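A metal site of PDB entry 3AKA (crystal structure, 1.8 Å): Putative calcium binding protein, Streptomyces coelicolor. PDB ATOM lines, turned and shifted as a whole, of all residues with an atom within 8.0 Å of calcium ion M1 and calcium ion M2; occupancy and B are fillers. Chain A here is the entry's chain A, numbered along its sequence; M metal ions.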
ATOM      1  N   VAL A 115      13.526  31.078   3.019  1.00  0.00           N
ATOM      2  CA  VAL A 115      14.725  31.933   3.048  1.00  0.00           C
ATOM      3  C   VAL A 115      15.966  31.036   3.233  1.00  0.00           C
ATOM      4  O   VAL A 115      15.926  30.108   4.057  1.00  0.00           O
ATOM      5  CB  VAL A 115      14.652  32.947   4.232  1.00  0.00           C
ATOM      6  CG1 VAL A 115      15.932  33.783   4.368  1.00  0.00           C
ATOM      7  CG2 VAL A 115      13.475  33.886   4.063  1.00  0.00           C
ATOM      8  N   VAL A 117      19.869  29.964   4.395  1.00  0.00           N
ATOM      9  CA  VAL A 117      20.718  30.275   5.538  1.00  0.00           C
ATOM     10  C   VAL A 117      21.575  31.529   5.286  1.00  0.00           C
ATOM     11  O   VAL A 117      21.654  32.395   6.174  1.00  0.00           O
ATOM     12  CB  VAL A 117      21.545  29.038   5.991  1.00  0.00           C
ATOM     13  CG1 VAL A 117      22.592  29.456   7.002  1.00  0.00           C
ATOM     14  CG2 VAL A 117      20.623  28.028   6.640  1.00  0.00           C
ATOM     15  N   ALA A 138      22.719  32.182  11.825  1.00  0.00           N
ATOM     16  CA  ALA A 138      21.862  31.733  10.722  1.00  0.00           C
ATOM     17  C   ALA A 138      21.843  30.211  10.647  1.00  0.00           C
ATOM     18  O   ALA A 138      20.771  29.621  10.548  1.00  0.00           O
ATOM     19  CB  ALA A 138      22.265  32.351   9.385  1.00  0.00           C
ATOM     20  N   ALA A 139      23.013  29.591  10.759  1.00  0.00           N
ATOM     21  CA  ALA A 139      23.160  28.140  10.722  1.00  0.00           C
ATOM     22  C   ALA A 139      22.338  27.501  11.832  1.00  0.00           C
ATOM     23  O   ALA A 139      21.602  26.517  11.602  1.00  0.00           O
ATOM     24  CB  ALA A 139      24.618  27.774  10.818  1.00  0.00           C
ATOM     25  N   LEU A 141      19.735  28.723  13.327  1.00  0.00           N
ATOM     26  CA  LEU A 141      18.299  28.922  13.157  1.00  0.00           C
ATOM     27  C   LEU A 141      17.691  27.797  12.319  1.00  0.00           C
ATOM     28  O   LEU A 141      16.504  27.501  12.453  1.00  0.00           O
ATOM     29  CB  LEU A 141      17.998  30.301  12.542  1.00  0.00           C
ATOM     30  CG  LEU A 141      18.238  31.495  13.485  1.00  0.00           C
ATOM     31  CD1 LEU A 141      18.278  32.830  12.760  1.00  0.00           C
ATOM     32  CD2 LEU A 141      17.217  31.526  14.591  1.00  0.00           C
ATOM     33  N   ASP A 142      18.503  27.173  11.465  1.00  0.00           N
ATOM     34  CA  ASP A 142      18.043  26.068  10.633  1.00  0.00           C
ATOM     35  C   ASP A 142      18.092  24.757  11.421  1.00  0.00           C
ATOM     36  O   ASP A 142      18.944  23.907  11.195  1.00  0.00           O
ATOM     37  CB  ASP A 142      18.868  25.985   9.350  1.00  0.00           C
ATOM     38  CG  ASP A 142      18.392  24.861   8.420  1.00  0.00           C
ATOM     39  OD1 ASP A 142      17.214  24.469   8.554  1.00  0.00           O
ATOM     40  OD2 ASP A 142      19.206  24.374   7.616  1.00  0.00           O
ATOM     41  N   THR A 143      17.171  24.608  12.358  1.00  0.00           N
ATOM     42  CA  THR A 143      17.174  23.482  13.314  1.00  0.00           C
ATOM     43  C   THR A 143      16.857  22.111  12.705  1.00  0.00           C
ATOM     44  O   THR A 143      17.144  21.077  13.332  1.00  0.00           O
ATOM     45  CB  THR A 143      16.200  23.743  14.462  1.00  0.00           C
ATOM     46  OG1 THR A 143      14.891  23.987  13.908  1.00  0.00           O
ATOM     47  CG2 THR A 143      16.673  24.929  15.320  1.00  0.00           C
ATOM     48  N   ASP A 144      16.215  22.074  11.543  1.00  0.00           N
ATOM     49  CA  ASP A 144      15.976  20.783  10.880  1.00  0.00           C
ATOM     50  C   ASP A 144      16.997  20.514   9.782  1.00  0.00           C
ATOM     51  O   ASP A 144      16.958  19.463   9.149  1.00  0.00           O
ATOM     52  CB  ASP A 144      14.528  20.584  10.404  1.00  0.00           C
ATOM     53  CG  ASP A 144      14.132  21.526   9.282  1.00  0.00           C
ATOM     54  OD1 ASP A 144      14.953  22.364   8.870  1.00  0.00           O
ATOM     55  OD2 ASP A 144      12.984  21.426   8.786  1.00  0.00           O
ATOM     56  N   GLY A 145      17.908  21.470   9.580  1.00  0.00           N
ATOM     57  CA  GLY A 145      19.024  21.302   8.631  1.00  0.00           C
ATOM     58  C   GLY A 145      18.721  21.181   7.136  1.00  0.00           C
ATOM     59  O   GLY A 145      19.530  20.625   6.358  1.00  0.00           O
ATOM     60  N   ASP A 146      17.564  21.687   6.713  1.00  0.00           N
ATOM     61  CA  ASP A 146      17.216  21.605   5.281  1.00  0.00           C
ATOM     62  C   ASP A 146      17.702  22.797   4.443  1.00  0.00           C
ATOM     63  O   ASP A 146      17.371  22.914   3.252  1.00  0.00           O
ATOM     64  CB  ASP A 146      15.718  21.358   5.062  1.00  0.00           C
ATOM     65  CG  ASP A 146      14.832  22.328   5.814  1.00  0.00           C
ATOM     66  OD1 ASP A 146      15.246  23.476   6.105  1.00  0.00           O
ATOM     67  OD2 ASP A 146      13.672  21.939   6.138  1.00  0.00           O
ATOM     68  N   GLY A 147      18.509  23.653   5.059  1.00  0.00           N
ATOM     69  CA  GLY A 147      19.095  24.814   4.366  1.00  0.00           C
ATOM     70  C   GLY A 147      18.078  25.940   4.122  1.00  0.00           C
ATOM     71  O   GLY A 147      18.340  26.893   3.374  1.00  0.00           O
ATOM     72  N   LYS A 148      16.916  25.798   4.739  1.00  0.00           N
ATOM     73  CA  LYS A 148      15.855  26.793   4.590  1.00  0.00           C
ATOM     74  C   LYS A 148      15.452  27.227   5.977  1.00  0.00           C
ATOM     75  O   LYS A 148      15.284  26.390   6.884  1.00  0.00           O
ATOM     76  CB  LYS A 148      14.673  26.225   3.833  1.00  0.00           C
ATOM     77  CG  LYS A 148      15.068  25.624   2.476  1.00  0.00           C
ATOM     78  CD  LYS A 148      13.868  25.145   1.712  1.00  0.00           C
ATOM     79  CE  LYS A 148      14.299  24.450   0.443  1.00  0.00           C
ATOM     80  NZ  LYS A 148      14.562  23.004   0.763  1.00  0.00           N
ATOM     81  N   VAL A 149      15.326  28.545   6.173  1.00  0.00           N
ATOM     82  CA  VAL A 149      14.963  29.081   7.469  1.00  0.00           C
ATOM     83  C   VAL A 149      13.551  29.657   7.374  1.00  0.00           C
ATOM     84  O   VAL A 149      13.242  30.427   6.457  1.00  0.00           O
ATOM     85  CB  VAL A 149      16.023  30.137   7.913  1.00  0.00           C
ATOM     86  CG1 VAL A 149      15.584  30.912   9.172  1.00  0.00           C
ATOM     87  CG2 VAL A 149      17.357  29.442   8.151  1.00  0.00           C
ATOM     88  N   GLY A 150      12.677  29.244   8.292  1.00  0.00           N
ATOM     89  CA  GLY A 150      11.267  29.645   8.188  1.00  0.00           C
ATOM     90  C   GLY A 150      10.663  30.225   9.463  1.00  0.00           C
ATOM     91  O   GLY A 150      11.312  30.230  10.514  1.00  0.00           O
ATOM     92  N   THR A 152       8.494  29.000  11.458  1.00  0.00           N
ATOM     93  CA  THR A 152       8.432  28.029  12.553  1.00  0.00           C
ATOM     94  C   THR A 152       9.761  27.866  13.290  1.00  0.00           C
ATOM     95  O   THR A 152       9.791  27.331  14.399  1.00  0.00           O
ATOM     96  CB  THR A 152       7.906  26.663  12.088  1.00  0.00           C
ATOM     97  OG1 THR A 152       8.775  26.177  11.059  1.00  0.00           O
ATOM     98  CG2 THR A 152       6.445  26.812  11.549  1.00  0.00           C
ATOM     99  N   GLU A 153      10.847  28.340  12.677  1.00  0.00           N
ATOM    100  CA  GLU A 153      12.169  28.339  13.321  1.00  0.00           C
ATOM    101  C   GLU A 153      12.506  29.679  13.993  1.00  0.00           C
ATOM    102  O   GLU A 153      12.974  29.714  15.139  1.00  0.00           O
ATOM    103  CB  GLU A 153      13.249  27.923  12.320  1.00  0.00           C
ATOM    104  CG  GLU A 153      13.089  26.435  11.880  1.00  0.00           C
ATOM    105  CD  GLU A 153      13.970  25.992  10.720  1.00  0.00           C
ATOM    106  OE1 GLU A 153      14.223  26.798   9.798  1.00  0.00           O
ATOM    107  OE2 GLU A 153      14.372  24.792  10.702  1.00  0.00           O
HETATM  108 CA    CA M   1      15.007  24.690   8.300  1.00  0.00          CA
HETATM  109 CA    CA M   2      12.381  22.477   7.378  1.00  0.00          CA
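The side-chain carboxylate (OD1) of Asp 142 lies close to the backbone NH (N) of Gly 145 (3.2 Å).
The side-chain carboxylate of Glu 153 lies close to the backbone NH of Gly 150 (3.3 Å).
The side-chain carboxylate of Glu 153 lies close to the backbone NH of Thr 143, at 3.3 Å.
The side-chain carboxylate (OD2) of Asp 142 sits at hydrogen-bond distance from the backbone NH (N) of Gly 147 (2.7 Å).
Within 4 Å of calcium ion M1: Asp 142, Asp 144, Asp 146, Lys 148 and Glu 153.
The nearest printed residue that does not touch calcium ion M1 is Val 149 (4.4 Å).
Within 4 Å of calcium ion M2: Asp 144 and Asp 146.
The nearest printed residue that does not touch calcium ion M2 is Glu 153 (4.5 Å).
Calcium ion M1 is bound by O of Lys 148 (2.2 Å), OD1 of Asp 142 (2.2 Å), OD1 of Asp 144 (2.4 Å), OE2 of Glu 153 (2.5 Å), OD1 of Asp 146 (2.5 Å) and OE1 of Glu 153 (2.7 Å).
Calcium ion M1 has six donor atoms within binding distance.
Calcium ion M2 is bound by the side-chain carboxylate (OD2) of Asp 144 (1.9 Å) and the side-chain carboxylate (OD2) of Asp 146 (1.9 Å).
Slightly farther from calcium ion M2 lies OD1 of Asp 144 (3.0 Å).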
